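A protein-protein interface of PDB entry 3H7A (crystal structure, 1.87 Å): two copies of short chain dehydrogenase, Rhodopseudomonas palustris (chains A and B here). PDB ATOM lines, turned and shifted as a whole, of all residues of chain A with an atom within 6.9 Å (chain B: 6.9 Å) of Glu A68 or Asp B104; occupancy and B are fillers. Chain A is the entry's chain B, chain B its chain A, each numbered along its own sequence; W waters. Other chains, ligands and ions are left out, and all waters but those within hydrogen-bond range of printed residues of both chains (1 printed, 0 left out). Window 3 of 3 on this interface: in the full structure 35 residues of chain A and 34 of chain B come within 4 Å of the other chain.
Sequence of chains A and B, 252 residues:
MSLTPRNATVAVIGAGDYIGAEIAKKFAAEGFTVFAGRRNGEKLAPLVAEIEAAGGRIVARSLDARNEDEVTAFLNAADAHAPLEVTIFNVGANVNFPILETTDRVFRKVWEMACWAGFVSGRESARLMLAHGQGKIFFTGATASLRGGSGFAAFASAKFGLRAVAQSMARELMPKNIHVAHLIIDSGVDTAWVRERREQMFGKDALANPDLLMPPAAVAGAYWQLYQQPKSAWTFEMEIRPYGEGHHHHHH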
ATOM      1  N   ASP A  64     -10.612   9.102  -6.367  1.00  0.00           N
ATOM      2  CA  ASP A  64      -9.541   9.556  -7.227  1.00  0.00           C
ATOM      3  C   ASP A  64     -10.130  10.544  -8.230  1.00  0.00           C
ATOM      4  O   ASP A  64     -10.774  10.158  -9.208  1.00  0.00           O
ATOM      5  CB  ASP A  64      -8.873   8.374  -7.927  1.00  0.00           C
ATOM      6  CG  ASP A  64      -7.716   8.797  -8.809  1.00  0.00           C
ATOM      7  OD1 ASP A  64      -7.113   9.867  -8.572  1.00  0.00           O
ATOM      8  OD2 ASP A  64      -7.405   8.040  -9.745  1.00  0.00           O
ATOM      9  N   ALA A  65      -9.868  11.825  -7.983  1.00  0.00           N
ATOM     10  CA  ALA A  65     -10.502  12.916  -8.714  1.00  0.00           C
ATOM     11  C   ALA A  65     -10.121  12.993 -10.189  1.00  0.00           C
ATOM     12  O   ALA A  65     -10.851  13.593 -10.971  1.00  0.00           O
ATOM     13  CB  ALA A  65     -10.252  14.240  -8.010  1.00  0.00           C
ATOM     14  N   ARG A  66      -9.014  12.353 -10.577  1.00  0.00           N
ATOM     15  CA  ARG A  66      -8.669  12.194 -11.993  1.00  0.00           C
ATOM     16  C   ARG A  66      -9.703  11.361 -12.740  1.00  0.00           C
ATOM     17  O   ARG A  66      -9.869  11.511 -13.945  1.00  0.00           O
ATOM     18  CB  ARG A  66      -7.311  11.527 -12.160  1.00  0.00           C
ATOM     19  CG  ARG A  66      -6.156  12.306 -11.604  1.00  0.00           C
ATOM     20  CD  ARG A  66      -4.884  11.502 -11.709  1.00  0.00           C
ATOM     21  NE  ARG A  66      -4.934  10.320 -10.858  1.00  0.00           N
ATOM     22  CZ  ARG A  66      -3.865   9.677 -10.407  1.00  0.00           C
ATOM     23  NH1 ARG A  66      -2.642  10.101 -10.715  1.00  0.00           N
ATOM     24  NH2 ARG A  66      -4.024   8.612  -9.634  1.00  0.00           N
ATOM     25  N   ASN A  67     -10.384  10.476 -12.016  1.00  0.00           N
ATOM     26  CA  ASN A  67     -11.350   9.555 -12.601  1.00  0.00           C
ATOM     27  C   ASN A  67     -12.737  10.211 -12.660  1.00  0.00           C
ATOM     28  O   ASN A  67     -13.410  10.370 -11.639  1.00  0.00           O
ATOM     29  CB  ASN A  67     -11.344   8.246 -11.793  1.00  0.00           C
ATOM     30  CG  ASN A  67     -12.052   7.089 -12.498  1.00  0.00           C
ATOM     31  OD1 ASN A  67     -13.087   7.250 -13.152  1.00  0.00           O
ATOM     32  ND2 ASN A  67     -11.493   5.896 -12.338  1.00  0.00           N
ATOM     33  N   GLU A  68     -13.156  10.584 -13.868  1.00  0.00           N
ATOM     34  CA  GLU A  68     -14.402  11.330 -14.077  1.00  0.00           C
ATOM     35  C   GLU A  68     -15.658  10.571 -13.662  1.00  0.00           C
ATOM     36  O   GLU A  68     -16.663  11.182 -13.316  1.00  0.00           O
ATOM     37  CB  GLU A  68     -14.524  11.803 -15.528  1.00  0.00           C
ATOM     38  CG  GLU A  68     -14.503  10.702 -16.591  1.00  0.00           C
ATOM     39  CD  GLU A  68     -13.099  10.319 -17.049  1.00  0.00           C
ATOM     40  OE1 GLU A  68     -12.107  10.710 -16.394  1.00  0.00           O
ATOM     41  OE2 GLU A  68     -12.998   9.617 -18.071  1.00  0.00           O
ATOM     42  N   ASP A  69     -15.584   9.241 -13.699  1.00  0.00           N
ATOM     43  CA  ASP A  69     -16.699   8.386 -13.321  1.00  0.00           C
ATOM     44  C   ASP A  69     -16.860   8.391 -11.811  1.00  0.00           C
ATOM     45  O   ASP A  69     -17.977   8.408 -11.309  1.00  0.00           O
ATOM     46  CB  ASP A  69     -16.482   6.968 -13.854  1.00  0.00           C
ATOM     47  CG  ASP A  69     -16.462   6.915 -15.378  1.00  0.00           C
ATOM     48  OD1 ASP A  69     -17.231   7.665 -16.024  1.00  0.00           O
ATOM     49  OD2 ASP A  69     -15.669   6.120 -15.931  1.00  0.00           O
ATOM     50  N   GLU A  70     -15.732   8.392 -11.104  1.00  0.00           N
ATOM     51  CA  GLU A  70     -15.701   8.495  -9.654  1.00  0.00           C
ATOM     52  C   GLU A  70     -16.155   9.870  -9.159  1.00  0.00           C
ATOM     53  O   GLU A  70     -16.859   9.956  -8.150  1.00  0.00           O
ATOM     54  CB  GLU A  70     -14.297   8.197  -9.125  1.00  0.00           C
ATOM     55  CG  GLU A  70     -13.888   6.730  -9.164  1.00  0.00           C
ATOM     56  CD  GLU A  70     -12.542   6.467  -8.464  1.00  0.00           C
ATOM     57  OE1 GLU A  70     -12.320   6.978  -7.343  1.00  0.00           O
ATOM     58  OE2 GLU A  70     -11.706   5.736  -9.038  1.00  0.00           O
ATOM     59  N   VAL A  71     -15.743  10.939  -9.846  1.00  0.00           N
ATOM     60  CA  VAL A  71     -16.177  12.306  -9.490  1.00  0.00           C
ATOM     61  C   VAL A  71     -17.686  12.425  -9.638  1.00  0.00           C
ATOM     62  O   VAL A  71     -18.363  12.909  -8.739  1.00  0.00           O
ATOM     63  CB  VAL A  71     -15.473  13.408 -10.357  1.00  0.00           C
ATOM     64  CG1 VAL A  71     -16.154  14.766 -10.204  1.00  0.00           C
ATOM     65  CG2 VAL A  71     -14.026  13.534  -9.972  1.00  0.00           C
ATOM     66  N   THR A  72     -18.197  11.960 -10.774  1.00  0.00           N
ATOM     67  CA  THR A  72     -19.624  11.991 -11.060  1.00  0.00           C
ATOM     68  C   THR A  72     -20.412  11.174 -10.023  1.00  0.00           C
ATOM     69  O   THR A  72     -21.463  11.613  -9.548  1.00  0.00           O
ATOM     70  CB  THR A  72     -19.867  11.517 -12.502  1.00  0.00           C
ATOM     71  OG1 THR A  72     -18.982  12.236 -13.369  1.00  0.00           O
ATOM     72  CG2 THR A  72     -21.306  11.762 -12.959  1.00  0.00           C
ATOM     73  N   ALA A  73     -19.889  10.011  -9.645  1.00  0.00           N
ATOM     74  CA  ALA A  73     -20.573   9.139  -8.695  1.00  0.00           C
ATOM     75  C   ALA A  73     -20.537   9.720  -7.298  1.00  0.00           C
ATOM     76  O   ALA A  73     -21.513   9.606  -6.569  1.00  0.00           O
ATOM     77  CB  ALA A  73     -19.978   7.724  -8.708  1.00  0.00           C
ATOM     78  N   TRP A 111      -2.104  17.948 -14.923  1.00  0.00           N
ATOM     79  CA  TRP A 111      -3.340  18.400 -15.541  1.00  0.00           C
ATOM     80  C   TRP A 111      -4.582  17.571 -15.141  1.00  0.00           C
ATOM     81  O   TRP A 111      -5.644  18.139 -14.831  1.00  0.00           O
ATOM     82  CB  TRP A 111      -3.198  18.414 -17.052  1.00  0.00           C
ATOM     83  CG  TRP A 111      -4.479  18.775 -17.743  1.00  0.00           C
ATOM     84  CD1 TRP A 111      -4.988  20.031 -17.918  1.00  0.00           C
ATOM     85  CD2 TRP A 111      -5.414  17.872 -18.354  1.00  0.00           C
ATOM     86  NE1 TRP A 111      -6.189  19.966 -18.591  1.00  0.00           N
ATOM     87  CE2 TRP A 111      -6.469  18.658 -18.878  1.00  0.00           C
ATOM     88  CE3 TRP A 111      -5.458  16.475 -18.511  1.00  0.00           C
ATOM     89  CZ2 TRP A 111      -7.553  18.099 -19.562  1.00  0.00           C
ATOM     90  CZ3 TRP A 111      -6.537  15.915 -19.191  1.00  0.00           C
ATOM     91  CH2 TRP A 111      -7.573  16.732 -19.709  1.00  0.00           C
ATOM     92  N   TRP A 116      -8.349  19.015 -14.995  1.00  0.00           N
ATOM     93  CA  TRP A 116      -9.360  18.105 -15.524  1.00  0.00           C
ATOM     94  C   TRP A 116     -10.338  17.736 -14.427  1.00  0.00           C
ATOM     95  O   TRP A 116     -11.540  17.862 -14.593  1.00  0.00           O
ATOM     96  CB  TRP A 116      -8.676  16.851 -16.085  1.00  0.00           C
ATOM     97  CG  TRP A 116      -9.584  15.657 -16.290  1.00  0.00           C
ATOM     98  CD1 TRP A 116      -9.613  14.505 -15.549  1.00  0.00           C
ATOM     99  CD2 TRP A 116     -10.585  15.504 -17.307  1.00  0.00           C
ATOM    100  NE1 TRP A 116     -10.575  13.650 -16.041  1.00  0.00           N
ATOM    101  CE2 TRP A 116     -11.183  14.239 -17.118  1.00  0.00           C
ATOM    102  CE3 TRP A 116     -11.034  16.315 -18.356  1.00  0.00           C
ATOM    103  CZ2 TRP A 116     -12.207  13.770 -17.938  1.00  0.00           C
ATOM    104  CZ3 TRP A 116     -12.044  15.847 -19.174  1.00  0.00           C
ATOM    105  CH2 TRP A 116     -12.623  14.583 -18.958  1.00  0.00           C
ATOM    106  N   PHE A 119     -12.598  20.628 -13.737  1.00  0.00           N
ATOM    107  CA  PHE A 119     -13.604  20.792 -14.783  1.00  0.00           C
ATOM    108  C   PHE A 119     -14.768  19.826 -14.578  1.00  0.00           C
ATOM    109  O   PHE A 119     -15.926  20.220 -14.700  1.00  0.00           O
ATOM    110  CB  PHE A 119     -12.990  20.597 -16.173  1.00  0.00           C
ATOM    111  CG  PHE A 119     -14.016  20.339 -17.263  1.00  0.00           C
ATOM    112  CD1 PHE A 119     -14.850  21.356 -17.703  1.00  0.00           C
ATOM    113  CD2 PHE A 119     -14.133  19.078 -17.834  1.00  0.00           C
ATOM    114  CE1 PHE A 119     -15.793  21.127 -18.698  1.00  0.00           C
ATOM    115  CE2 PHE A 119     -15.079  18.829 -18.825  1.00  0.00           C
ATOM    116  CZ  PHE A 119     -15.909  19.859 -19.257  1.00  0.00           C
ATOM    117  N   VAL A 120     -14.458  18.571 -14.263  1.00  0.00           N
ATOM    118  CA  VAL A 120     -15.495  17.550 -14.151  1.00  0.00           C
ATOM    119  C   VAL A 120     -16.323  17.809 -12.909  1.00  0.00           C
ATOM    120  O   VAL A 120     -17.554  17.821 -12.986  1.00  0.00           O
ATOM    121  CB  VAL A 120     -14.934  16.111 -14.202  1.00  0.00           C
ATOM    122  CG1 VAL A 120     -16.048  15.076 -14.008  1.00  0.00           C
ATOM    123  CG2 VAL A 120     -14.223  15.873 -15.549  1.00  0.00           C
ATOM    124  N   ARG A 123     -18.525  20.998 -13.652  1.00  0.00           N
ATOM    125  CA  ARG A 123     -19.608  20.686 -14.587  1.00  0.00           C
ATOM    126  C   ARG A 123     -20.697  19.823 -13.963  1.00  0.00           C
ATOM    127  O   ARG A 123     -21.893  20.113 -14.102  1.00  0.00           O
ATOM    128  CB  ARG A 123     -19.052  19.988 -15.838  1.00  0.00           C
ATOM    129  CG  ARG A 123     -20.106  19.765 -16.927  1.00  0.00           C
ATOM    130  CD  ARG A 123     -19.629  18.774 -17.983  1.00  0.00           C
ATOM    131  NE  ARG A 123     -19.366  17.449 -17.417  1.00  0.00           N
ATOM    132  CZ  ARG A 123     -18.606  16.520 -17.986  1.00  0.00           C
ATOM    133  NH1 ARG A 123     -18.019  16.760 -19.156  1.00  0.00           N
ATOM    134  NH2 ARG A 123     -18.430  15.348 -17.386  1.00  0.00           N
ATOM    135  N   GLU A 124     -20.280  18.780 -13.253  1.00  0.00           N
ATOM    136  CA  GLU A 124     -21.233  17.889 -12.603  1.00  0.00           C
ATOM    137  C   GLU A 124     -21.928  18.528 -11.405  1.00  0.00           C
ATOM    138  O   GLU A 124     -23.107  18.275 -11.195  1.00  0.00           O
ATOM    139  CB  GLU A 124     -20.586  16.540 -12.247  1.00  0.00           C
ATOM    140  CG  GLU A 124     -20.119  15.743 -13.477  1.00  0.00           C
ATOM    141  CD  GLU A 124     -21.201  15.598 -14.563  1.00  0.00           C
ATOM    142  OE1 GLU A 124     -22.309  15.093 -14.260  1.00  0.00           O
ATOM    143  OE2 GLU A 124     -20.937  15.990 -15.724  1.00  0.00           O
ATOM    144  N   THR B 102     -20.310  20.832 -22.573  1.00  0.00           N
ATOM    145  CA  THR B 102     -18.890  20.631 -22.833  1.00  0.00           C
ATOM    146  C   THR B 102     -18.578  19.223 -22.404  1.00  0.00           C
ATOM    147  O   THR B 102     -18.572  18.923 -21.206  1.00  0.00           O
ATOM    148  CB  THR B 102     -18.023  21.650 -22.076  1.00  0.00           C
ATOM    149  OG1 THR B 102     -18.511  22.966 -22.342  1.00  0.00           O
ATOM    150  CG2 THR B 102     -16.559  21.565 -22.512  1.00  0.00           C
ATOM    151  N   THR B 103     -18.359  18.354 -23.391  1.00  0.00           N
ATOM    152  CA  THR B 103     -18.210  16.921 -23.140  1.00  0.00           C
ATOM    153  C   THR B 103     -16.796  16.635 -22.678  1.00  0.00           C
ATOM    154  O   THR B 103     -15.912  17.481 -22.829  1.00  0.00           O
ATOM    155  CB  THR B 103     -18.510  16.085 -24.389  1.00  0.00           C
ATOM    156  OG1 THR B 103     -17.656  16.496 -25.462  1.00  0.00           O
ATOM    157  CG2 THR B 103     -19.945  16.278 -24.826  1.00  0.00           C
ATOM    158  N   ASP B 104     -16.598  15.445 -22.113  1.00  0.00           N
ATOM    159  CA  ASP B 104     -15.272  14.942 -21.790  1.00  0.00           C
ATOM    160  C   ASP B 104     -14.373  14.964 -23.021  1.00  0.00           C
ATOM    161  O   ASP B 104     -13.219  15.415 -22.944  1.00  0.00           O
ATOM    162  CB  ASP B 104     -15.356  13.517 -21.240  1.00  0.00           C
ATOM    163  CG  ASP B 104     -16.069  13.431 -19.897  1.00  0.00           C
ATOM    164  OD1 ASP B 104     -16.410  14.473 -19.284  1.00  0.00           O
ATOM    165  OD2 ASP B 104     -16.269  12.290 -19.441  1.00  0.00           O
ATOM    166  N   ARG B 105     -14.909  14.507 -24.151  1.00  0.00           N
ATOM    167  CA  ARG B 105     -14.137  14.386 -25.380  1.00  0.00           C
ATOM    168  C   ARG B 105     -13.643  15.738 -25.867  1.00  0.00           C
ATOM    169  O   ARG B 105     -12.495  15.868 -26.275  1.00  0.00           O
ATOM    170  CB  ARG B 105     -14.957  13.703 -26.479  1.00  0.00           C
ATOM    171  CG  ARG B 105     -14.106  13.152 -27.625  1.00  0.00           C
ATOM    172  CD  ARG B 105     -14.943  12.743 -28.852  1.00  0.00           C
ATOM    173  NE  ARG B 105     -15.336  13.903 -29.657  1.00  0.00           N
ATOM    174  CZ  ARG B 105     -14.608  14.428 -30.644  1.00  0.00           C
ATOM    175  NH1 ARG B 105     -13.431  13.901 -30.980  1.00  0.00           N
ATOM    176  NH2 ARG B 105     -15.058  15.487 -31.302  1.00  0.00           N
ATOM    177  N   VAL B 106     -14.522  16.734 -25.834  1.00  0.00           N
ATOM    178  CA  VAL B 106     -14.194  18.095 -26.275  1.00  0.00           C
ATOM    179  C   VAL B 106     -13.178  18.783 -25.359  1.00  0.00           C
ATOM    180  O   VAL B 106     -12.206  19.346 -25.854  1.00  0.00           O
ATOM    181  CB  VAL B 106     -15.479  18.940 -26.488  1.00  0.00           C
ATOM    182  CG1 VAL B 106     -15.183  20.437 -26.577  1.00  0.00           C
ATOM    183  CG2 VAL B 106     -16.201  18.467 -27.740  1.00  0.00           C
ATOM    184  N   PHE B 107     -13.377  18.713 -24.038  1.00  0.00           N
ATOM    185  CA  PHE B 107     -12.425  19.332 -23.108  1.00  0.00           C
ATOM    186  C   PHE B 107     -11.020  18.760 -23.241  1.00  0.00           C
ATOM    187  O   PHE B 107     -10.048  19.504 -23.245  1.00  0.00           O
ATOM    188  CB  PHE B 107     -12.892  19.187 -21.660  1.00  0.00           C
ATOM    189  CG  PHE B 107     -12.145  20.077 -20.673  1.00  0.00           C
ATOM    190  CD1 PHE B 107     -12.528  21.399 -20.480  1.00  0.00           C
ATOM    191  CD2 PHE B 107     -11.080  19.586 -19.935  1.00  0.00           C
ATOM    192  CE1 PHE B 107     -11.864  22.228 -19.580  1.00  0.00           C
ATOM    193  CE2 PHE B 107     -10.407  20.407 -19.019  1.00  0.00           C
ATOM    194  CZ  PHE B 107     -10.804  21.728 -18.842  1.00  0.00           C
ATOM    195  N   ARG B 108     -10.923  17.436 -23.339  1.00  0.00           N
ATOM    196  CA  ARG B 108      -9.641  16.751 -23.477  1.00  0.00           C
ATOM    197  C   ARG B 108      -8.973  17.057 -24.830  1.00  0.00           C
ATOM    198  O   ARG B 108      -7.791  17.415 -24.874  1.00  0.00           O
ATOM    199  CB  ARG B 108      -9.848  15.243 -23.297  1.00  0.00           C
ATOM    200  CG  ARG B 108      -8.570  14.430 -23.167  1.00  0.00           C
ATOM    201  CD  ARG B 108      -8.874  12.944 -23.070  1.00  0.00           C
ATOM    202  NE  ARG B 108      -9.602  12.579 -21.849  1.00  0.00           N
ATOM    203  CZ  ARG B 108     -10.895  12.251 -21.800  1.00  0.00           C
ATOM    204  NH1 ARG B 108     -11.444  11.924 -20.639  1.00  0.00           N
ATOM    205  NH2 ARG B 108     -11.642  12.245 -22.901  1.00  0.00           N
ATOM    206  N   LYS B 109      -9.722  16.920 -25.926  1.00  0.00           N
ATOM    207  CA  LYS B 109      -9.188  17.182 -27.258  1.00  0.00           C
ATOM    208  C   LYS B 109      -8.658  18.614 -27.361  1.00  0.00           C
ATOM    209  O   LYS B 109      -7.590  18.841 -27.927  1.00  0.00           O
ATOM    210  CB  LYS B 109     -10.257  16.926 -28.335  1.00  0.00           C
ATOM    211  CG  LYS B 109      -9.762  17.089 -29.774  1.00  0.00           C
ATOM    212  CD  LYS B 109     -10.835  16.736 -30.812  1.00  0.00           C
ATOM    213  CE  LYS B 109     -10.232  16.697 -32.220  1.00  0.00           C
ATOM    214  NZ  LYS B 109     -11.182  16.164 -33.248  1.00  0.00           N
ATOM    215  N   VAL B 110      -9.398  19.573 -26.797  1.00  0.00           N
ATOM    216  CA  VAL B 110      -8.978  20.970 -26.826  1.00  0.00           C
ATOM    217  C   VAL B 110      -7.659  21.152 -26.051  1.00  0.00           C
ATOM    218  O   VAL B 110      -6.727  21.747 -26.578  1.00  0.00           O
ATOM    219  CB  VAL B 110     -10.112  21.959 -26.431  1.00  0.00           C
ATOM    220  CG1 VAL B 110      -9.586  23.377 -26.337  1.00  0.00           C
ATOM    221  CG2 VAL B 110     -11.228  21.928 -27.490  1.00  0.00           C
HETATM  222  O   HOH W   1     -15.045  10.296 -20.254  1.00  0.00           O
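The backbone carbonyl oxygen (O) of Thr B102 lies within hydrogen-bond range of the guanidinium group (NH1) of Arg A123.
OD1 of Asp B104 is in salt-bridge range of NH1 of Arg A123 (2.8 Å).
NH1 of Arg B108 lies within salt-bridge range of OE2 of Glu A68.
The side-chain hydroxyl (OG1) of Thr B103 is in hydrogen-bond range of the backbone NH (N) of Val B106, at 3.2 Å.
The indole nitrogen (NE1) of Trp A116 sits at hydrogen-bond distance from the backbone carbonyl oxygen (O) of Arg A66 (3.1 Å).
The backbone carbonyl oxygen of Glu A68 lies within hydrogen-bond range of the side-chain hydroxyl of Thr A72, 2.5 Å away.
OE1 of Glu A68 lies within hydrogen-bond range of NE1 of Trp A116, at 3.3 Å.
N of Trp A116 sits at hydrogen-bond distance from O of Trp A111 (2.8 Å).
The side-chain carboxylate (OE2) of Glu A124 is in salt-bridge range of the guanidinium group (NE) of Arg A123, at 2.7 Å.
Glu A68 touches Asp B104.
Trp A111 touches Phe B107.
Trp A116 touches Asp B104.
Trp A116 touches Phe B107.
NH1 of Arg B108 touches CZ2 of Trp A116 (3.4 Å).
CZ of Phe A119 touches O of Thr B102 (3.4 Å).
Phe B107 touches Phe A119 (CB to CE2, 3.6 Å).
Arg A123 touches Thr B103.
Of the printed residues of chain B, Glu A68 touches Asp B104 (3.7 Å) and Arg B108 (3.8 Å).
Asp B104 touches just these residues of chain A: Glu A68 (3.7 Å), Trp A116 (3.7 Å) and Arg A123 (2.8 Å).
Of the printed residues of chain B, Phe A119 touches Thr B102 (3.4 Å) and Phe B107 (3.6 Å).
Of the printed residues of chain A, Phe B107 touches Trp A111 (3.7 Å), Trp A116 (3.6 Å) and Phe A119 (3.6 Å).
Printed residues of chain A within 4 Å of Arg B108: Glu A68 and Trp A116.
Of the printed residues of chain A, Thr B102 touches Phe A119 (3.4 Å) and Arg A123 (3.0 Å).
Of the printed residues of chain B, Trp A116 touches Asp B104, Phe B107 and Arg B108.
Arg B105 touches none of the printed residues of chain A.
The nearest printed residue of chain B that does not touch Glu A68 is Arg B105 (8.0 Å).
Of the 16 printed residues of chain A, 5 touch a printed residue of chain B.
Hydrophobic or aromatic side chains of chain A within 4 Å of the printed part of chain B: Trp A111, Trp A116 and Phe A119.
Among the printed residues, 11 pairs touch across the chains.
No position is printed for both chains.
Of the 11 pairs that touch across the chains among the printed residues, none has its exchanged pair printed and touching as well.
Water W1 bridges the side-chain carboxylate (OD2) of Asp B104 (2.5 Å) and the side-chain carboxylate (OE2) of Glu A68 (3.1 Å).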
